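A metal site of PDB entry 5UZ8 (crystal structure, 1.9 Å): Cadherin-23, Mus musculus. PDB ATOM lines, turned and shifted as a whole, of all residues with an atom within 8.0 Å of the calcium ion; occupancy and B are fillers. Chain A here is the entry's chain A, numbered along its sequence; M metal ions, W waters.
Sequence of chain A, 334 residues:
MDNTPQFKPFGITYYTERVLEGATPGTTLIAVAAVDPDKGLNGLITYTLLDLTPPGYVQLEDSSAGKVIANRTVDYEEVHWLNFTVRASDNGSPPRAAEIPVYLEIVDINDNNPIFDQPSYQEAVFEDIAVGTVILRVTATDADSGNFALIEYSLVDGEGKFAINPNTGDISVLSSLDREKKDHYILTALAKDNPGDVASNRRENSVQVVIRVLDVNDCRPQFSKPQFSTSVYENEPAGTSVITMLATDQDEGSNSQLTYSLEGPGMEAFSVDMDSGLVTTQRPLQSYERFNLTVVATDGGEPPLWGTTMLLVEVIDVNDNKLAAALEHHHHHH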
ATOM      1  N   ASP A   2     -23.855 -17.300   2.217  1.00  0.00           N
ATOM      2  CA  ASP A   2     -22.382 -17.347   1.926  1.00  0.00           C
ATOM      3  C   ASP A   2     -21.681 -15.968   1.974  1.00  0.00           C
ATOM      4  O   ASP A   2     -20.712 -15.713   1.251  1.00  0.00           O
ATOM      5  CB  ASP A   2     -22.122 -18.063   0.588  1.00  0.00           C
ATOM      6  CG  ASP A   2     -22.924 -17.477  -0.562  1.00  0.00           C
ATOM      7  OD1 ASP A   2     -23.525 -16.377  -0.386  1.00  0.00           O
ATOM      8  OD2 ASP A   2     -22.980 -18.118  -1.637  1.00  0.00           O
ATOM      9  N   ASN A   3     -22.181 -15.079   2.835  1.00  0.00           N
ATOM     10  CA  ASN A   3     -21.573 -13.771   3.044  1.00  0.00           C
ATOM     11  C   ASN A   3     -20.703 -13.797   4.318  1.00  0.00           C
ATOM     12  O   ASN A   3     -21.103 -14.338   5.329  1.00  0.00           O
ATOM     13  CB  ASN A   3     -22.666 -12.693   3.148  1.00  0.00           C
ATOM     14  CG  ASN A   3     -23.452 -12.537   1.861  1.00  0.00           C
ATOM     15  OD1 ASN A   3     -22.972 -11.949   0.897  1.00  0.00           O
ATOM     16  ND2 ASN A   3     -24.658 -13.099   1.823  1.00  0.00           N
ATOM     17  N   THR A   4     -19.485 -13.254   4.226  1.00  0.00           N
ATOM     18  CA  THR A   4     -18.594 -13.091   5.373  1.00  0.00           C
ATOM     19  C   THR A   4     -19.019 -11.874   6.203  1.00  0.00           C
ATOM     20  O   THR A   4     -19.435 -10.868   5.633  1.00  0.00           O
ATOM     21  CB  THR A   4     -17.162 -12.886   4.851  1.00  0.00           C
ATOM     22  OG1 THR A   4     -16.858 -13.970   3.983  1.00  0.00           O
ATOM     23  CG2 THR A   4     -16.135 -12.817   5.975  1.00  0.00           C
ATOM     24  N   PRO A   5     -18.922 -11.950   7.549  1.00  0.00           N
ATOM     25  CA  PRO A   5     -19.218 -10.757   8.321  1.00  0.00           C
ATOM     26  C   PRO A   5     -18.360  -9.559   7.913  1.00  0.00           C
ATOM     27  O   PRO A   5     -17.159  -9.728   7.596  1.00  0.00           O
ATOM     28  CB  PRO A   5     -18.902 -11.183   9.762  1.00  0.00           C
ATOM     29  CG  PRO A   5     -19.160 -12.666   9.760  1.00  0.00           C
ATOM     30  CD  PRO A   5     -18.709 -13.127   8.413  1.00  0.00           C
ATOM     31  N   VAL A  35     -21.745  -7.030  10.682  1.00  0.00           N
ATOM     32  CA  VAL A  35     -23.030  -7.498  10.174  1.00  0.00           C
ATOM     33  C   VAL A  35     -22.806  -8.646   9.206  1.00  0.00           C
ATOM     34  O   VAL A  35     -21.776  -8.742   8.576  1.00  0.00           O
ATOM     35  CB  VAL A  35     -23.834  -6.384   9.480  1.00  0.00           C
ATOM     36  CG1 VAL A  35     -24.204  -5.285  10.477  1.00  0.00           C
ATOM     37  CG2 VAL A  35     -23.055  -5.816   8.308  1.00  0.00           C
ATOM     38  N   ASP A  36     -23.798  -9.516   9.130  1.00  0.00           N
ATOM     39  CA  ASP A  36     -23.794 -10.606   8.195  1.00  0.00           C
ATOM     40  C   ASP A  36     -25.220 -10.685   7.713  1.00  0.00           C
ATOM     41  O   ASP A  36     -26.113 -10.911   8.526  1.00  0.00           O
ATOM     42  CB  ASP A  36     -23.380 -11.892   8.908  1.00  0.00           C
ATOM     43  CG  ASP A  36     -23.239 -13.055   7.960  1.00  0.00           C
ATOM     44  OD1 ASP A  36     -24.202 -13.395   7.234  1.00  0.00           O
ATOM     45  OD2 ASP A  36     -22.134 -13.652   7.937  1.00  0.00           O
ATOM     46  N   PRO A  37     -25.452 -10.481   6.414  1.00  0.00           N
ATOM     47  CA  PRO A  37     -26.854 -10.506   5.926  1.00  0.00           C
ATOM     48  C   PRO A  37     -27.611 -11.868   6.047  1.00  0.00           C
ATOM     49  O   PRO A  37     -28.843 -11.874   6.126  1.00  0.00           O
ATOM     50  CB  PRO A  37     -26.730 -10.039   4.454  1.00  0.00           C
ATOM     51  CG  PRO A  37     -25.309 -10.293   4.088  1.00  0.00           C
ATOM     52  CD  PRO A  37     -24.493 -10.148   5.337  1.00  0.00           C
ATOM     53  N   ASP A  38     -26.873 -12.979   6.125  1.00  0.00           N
ATOM     54  CA  ASP A  38     -27.440 -14.338   5.992  1.00  0.00           C
ATOM     55  C   ASP A  38     -28.390 -14.750   7.127  1.00  0.00           C
ATOM     56  O   ASP A  38     -28.443 -14.115   8.170  1.00  0.00           O
ATOM     57  CB  ASP A  38     -26.320 -15.378   5.897  1.00  0.00           C
ATOM     58  CG  ASP A  38     -25.333 -15.095   4.761  1.00  0.00           C
ATOM     59  OD1 ASP A  38     -25.771 -14.526   3.732  1.00  0.00           O
ATOM     60  OD2 ASP A  38     -24.132 -15.430   4.917  1.00  0.00           O
ATOM     61  N   LYS A  39     -29.134 -15.829   6.887  1.00  0.00           N
ATOM     62  CA  LYS A  39     -30.175 -16.307   7.816  1.00  0.00           C
ATOM     63  C   LYS A  39     -29.602 -17.283   8.860  1.00  0.00           C
ATOM     64  O   LYS A  39     -28.708 -18.082   8.539  1.00  0.00           O
ATOM     65  CB  LYS A  39     -31.309 -16.993   7.034  1.00  0.00           C
ATOM     66  CG  LYS A  39     -30.985 -18.403   6.528  1.00  0.00           C
ATOM     67  CD  LYS A  39     -31.995 -18.887   5.495  1.00  0.00           C
ATOM     68  CE  LYS A  39     -31.603 -20.246   4.937  1.00  0.00           C
ATOM     69  NZ  LYS A  39     -32.490 -20.664   3.818  1.00  0.00           N
ATOM     70  N   GLY A  40     -30.138 -17.213  10.077  1.00  0.00           N
ATOM     71  CA  GLY A  40     -29.869 -18.215  11.128  1.00  0.00           C
ATOM     72  C   GLY A  40     -28.411 -18.304  11.561  1.00  0.00           C
ATOM     73  O   GLY A  40     -27.739 -17.270  11.726  1.00  0.00           O
ATOM     74  N   LEU A  41     -27.924 -19.530  11.730  1.00  0.00           N
ATOM     75  CA  LEU A  41     -26.525 -19.776  12.110  1.00  0.00           C
ATOM     76  C   LEU A  41     -25.527 -19.211  11.099  1.00  0.00           C
ATOM     77  O   LEU A  41     -24.426 -18.778  11.484  1.00  0.00           O
ATOM     78  CB  LEU A  41     -26.270 -21.288  12.295  1.00  0.00           C
ATOM     79  CG  LEU A  41     -26.943 -21.991  13.478  1.00  0.00           C
ATOM     80  CD1 LEU A  41     -26.710 -23.504  13.405  1.00  0.00           C
ATOM     81  CD2 LEU A  41     -26.466 -21.419  14.806  1.00  0.00           C
ATOM     82  N   ASN A  42     -25.915 -19.169   9.820  1.00  0.00           N
ATOM     83  CA  ASN A  42     -25.085 -18.549   8.769  1.00  0.00           C
ATOM     84  C   ASN A  42     -24.890 -17.028   8.946  1.00  0.00           C
ATOM     85  O   ASN A  42     -23.914 -16.477   8.444  1.00  0.00           O
ATOM     86  CB  ASN A  42     -25.645 -18.834   7.376  1.00  0.00           C
ATOM     87  CG  ASN A  42     -25.599 -20.310   7.021  1.00  0.00           C
ATOM     88  OD1 ASN A  42     -24.534 -20.933   7.044  1.00  0.00           O
ATOM     89  ND2 ASN A  42     -26.747 -20.868   6.675  1.00  0.00           N
ATOM     90  N   GLY A  43     -25.838 -16.367   9.615  1.00  0.00           N
ATOM     91  CA  GLY A  43     -25.722 -14.928   9.898  1.00  0.00           C
ATOM     92  C   GLY A  43     -25.675 -14.559  11.365  1.00  0.00           C
ATOM     93  O   GLY A  43     -25.795 -13.372  11.701  1.00  0.00           O
ATOM     94  N   LEU A  44     -25.482 -15.546  12.246  1.00  0.00           N
ATOM     95  CA  LEU A  44     -25.339 -15.308  13.691  1.00  0.00           C
ATOM     96  C   LEU A  44     -23.873 -15.045  14.053  1.00  0.00           C
ATOM     97  O   LEU A  44     -23.034 -15.946  13.925  1.00  0.00           O
ATOM     98  CB  LEU A  44     -25.847 -16.528  14.452  1.00  0.00           C
ATOM     99  CG  LEU A  44     -25.839 -16.488  15.969  1.00  0.00           C
ATOM    100  CD1 LEU A  44     -26.458 -15.194  16.494  1.00  0.00           C
ATOM    101  CD2 LEU A  44     -26.604 -17.712  16.477  1.00  0.00           C
ATOM    102  N   ILE A  45     -23.567 -13.836  14.508  1.00  0.00           N
ATOM    103  CA  ILE A  45     -22.183 -13.435  14.696  1.00  0.00           C
ATOM    104  C   ILE A  45     -21.730 -13.631  16.120  1.00  0.00           C
ATOM    105  O   ILE A  45     -22.374 -13.155  17.041  1.00  0.00           O
ATOM    106  CB  ILE A  45     -21.942 -11.960  14.272  1.00  0.00           C
ATOM    107  CG1 ILE A  45     -22.300 -11.811  12.778  1.00  0.00           C
ATOM    108  CG2 ILE A  45     -20.491 -11.535  14.539  1.00  0.00           C
ATOM    109  CD1 ILE A  45     -22.423 -10.385  12.334  1.00  0.00           C
ATOM    110  N   SER A  89     -17.195 -13.882  13.728  1.00  0.00           N
ATOM    111  CA  SER A  89     -17.357 -15.148  12.988  1.00  0.00           C
ATOM    112  C   SER A  89     -18.853 -15.451  12.889  1.00  0.00           C
ATOM    113  O   SER A  89     -19.588 -15.258  13.853  1.00  0.00           O
ATOM    114  CB  SER A  89     -16.656 -16.285  13.732  1.00  0.00           C
ATOM    115  OG  SER A  89     -16.802 -17.512  12.999  1.00  0.00           O
ATOM    116  N   ASP A  90     -19.321 -15.897  11.730  1.00  0.00           N
ATOM    117  CA  ASP A  90     -20.674 -16.417  11.680  1.00  0.00           C
ATOM    118  C   ASP A  90     -20.601 -17.819  12.207  1.00  0.00           C
ATOM    119  O   ASP A  90     -19.519 -18.331  12.468  1.00  0.00           O
ATOM    120  CB  ASP A  90     -21.328 -16.319  10.296  1.00  0.00           C
ATOM    121  CG  ASP A  90     -20.671 -17.209   9.223  1.00  0.00           C
ATOM    122  OD1 ASP A  90     -20.111 -18.295   9.529  1.00  0.00           O
ATOM    123  OD2 ASP A  90     -20.730 -16.816   8.041  1.00  0.00           O
ATOM    124  N   ASN A  91     -21.753 -18.453  12.373  1.00  0.00           N
ATOM    125  CA  ASN A  91     -21.765 -19.787  12.951  1.00  0.00           C
ATOM    126  C   ASN A  91     -22.153 -20.826  11.903  1.00  0.00           C
ATOM    127  O   ASN A  91     -22.700 -21.856  12.232  1.00  0.00           O
ATOM    128  CB  ASN A  91     -22.684 -19.816  14.177  1.00  0.00           C
ATOM    129  CG  ASN A  91     -22.012 -19.211  15.402  1.00  0.00           C
ATOM    130  OD1 ASN A  91     -21.553 -19.949  16.275  1.00  0.00           O
ATOM    131  ND2 ASN A  91     -21.915 -17.878  15.454  1.00  0.00           N
ATOM    132  N   GLY A  92     -21.808 -20.548  10.636  1.00  0.00           N
ATOM    133  CA  GLY A  92     -22.100 -21.455   9.533  1.00  0.00           C
ATOM    134  C   GLY A  92     -21.180 -22.653   9.506  1.00  0.00           C
ATOM    135  O   GLY A  92     -20.249 -22.770  10.314  1.00  0.00           O
ATOM    136  N   PRO A  94     -18.869 -24.507   7.339  1.00  0.00           N
ATOM    137  CA  PRO A  94     -17.534 -23.928   7.564  1.00  0.00           C
ATOM    138  C   PRO A  94     -17.795 -22.465   7.922  1.00  0.00           C
ATOM    139  O   PRO A  94     -18.418 -21.755   7.124  1.00  0.00           O
ATOM    140  CB  PRO A  94     -16.849 -24.083   6.211  1.00  0.00           C
ATOM    141  CG  PRO A  94     -17.958 -24.120   5.211  1.00  0.00           C
ATOM    142  CD  PRO A  94     -19.219 -24.544   5.907  1.00  0.00           C
ATOM    143  N   PRO A  95     -17.396 -22.027   9.133  1.00  0.00           N
ATOM    144  CA  PRO A  95     -17.709 -20.640   9.472  1.00  0.00           C
ATOM    145  C   PRO A  95     -16.897 -19.647   8.637  1.00  0.00           C
ATOM    146  O   PRO A  95     -15.798 -19.974   8.195  1.00  0.00           O
ATOM    147  CB  PRO A  95     -17.321 -20.542  10.963  1.00  0.00           C
ATOM    148  CG  PRO A  95     -16.263 -21.573  11.123  1.00  0.00           C
ATOM    149  CD  PRO A  95     -16.655 -22.697  10.218  1.00  0.00           C
ATOM    150  N   ARG A  96     -17.468 -18.477   8.390  1.00  0.00           N
ATOM    151  CA  ARG A  96     -16.751 -17.380   7.774  1.00  0.00           C
ATOM    152  C   ARG A  96     -16.571 -16.312   8.829  1.00  0.00           C
ATOM    153  O   ARG A  96     -17.453 -16.074   9.670  1.00  0.00           O
ATOM    154  CB  ARG A  96     -17.528 -16.817   6.594  1.00  0.00           C
ATOM    155  CG  ARG A  96     -17.754 -17.781   5.441  1.00  0.00           C
ATOM    156  CD  ARG A  96     -18.574 -17.096   4.349  1.00  0.00           C
ATOM    157  NE  ARG A  96     -18.598 -17.835   3.096  1.00  0.00           N
ATOM    158  CZ  ARG A  96     -19.354 -18.896   2.838  1.00  0.00           C
ATOM    159  NH1 ARG A  96     -19.299 -19.488   1.636  1.00  0.00           N
ATOM    160  NH2 ARG A  96     -20.176 -19.391   3.764  1.00  0.00           N
ATOM    161  N   ALA A  97     -15.428 -15.652   8.786  1.00  0.00           N
ATOM    162  CA  ALA A  97     -15.079 -14.696   9.797  1.00  0.00           C
ATOM    163  C   ALA A  97     -14.275 -13.565   9.201  1.00  0.00           C
ATOM    164  O   ALA A  97     -13.709 -13.683   8.138  1.00  0.00           O
ATOM    165  CB  ALA A  97     -14.308 -15.382  10.912  1.00  0.00           C
HETATM  166 CA    CA M   1     -22.453 -15.592   6.748  1.00  0.00          CA
HETATM  167  O   HOH W   1     -22.337 -17.748   5.664  1.00  0.00           O
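The backbone carbonyl oxygen of Arg 96 is in hydrogen-bond range of the backbone NH of Asp 90, at 2.8 Å. OD1 of Asp 90 sits at hydrogen-bond distance from N of Gly 92 (3.0 Å). OD2 of Asp 38 lies close to N of Asp 2 (3.3 Å).
Of the 23 residues printed, 5 come within 4 Å of the calcium ion. The nearest printed residue that does not touch the calcium ion is Gly 43 (4.5 Å).
The calcium ion is bound by OD2 of Asp 36 (2.3 Å), O of Asn 3 (2.3 Å), O of Asn 42 (2.4 Å), water W1 (2.4 Å), OD2 of Asp 90 (2.5 Å), OD2 of Asp 38 (2.5 Å) and OD1 of Asp 36 (2.8 Å). The calcium ion has seven donor atoms within binding distance.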
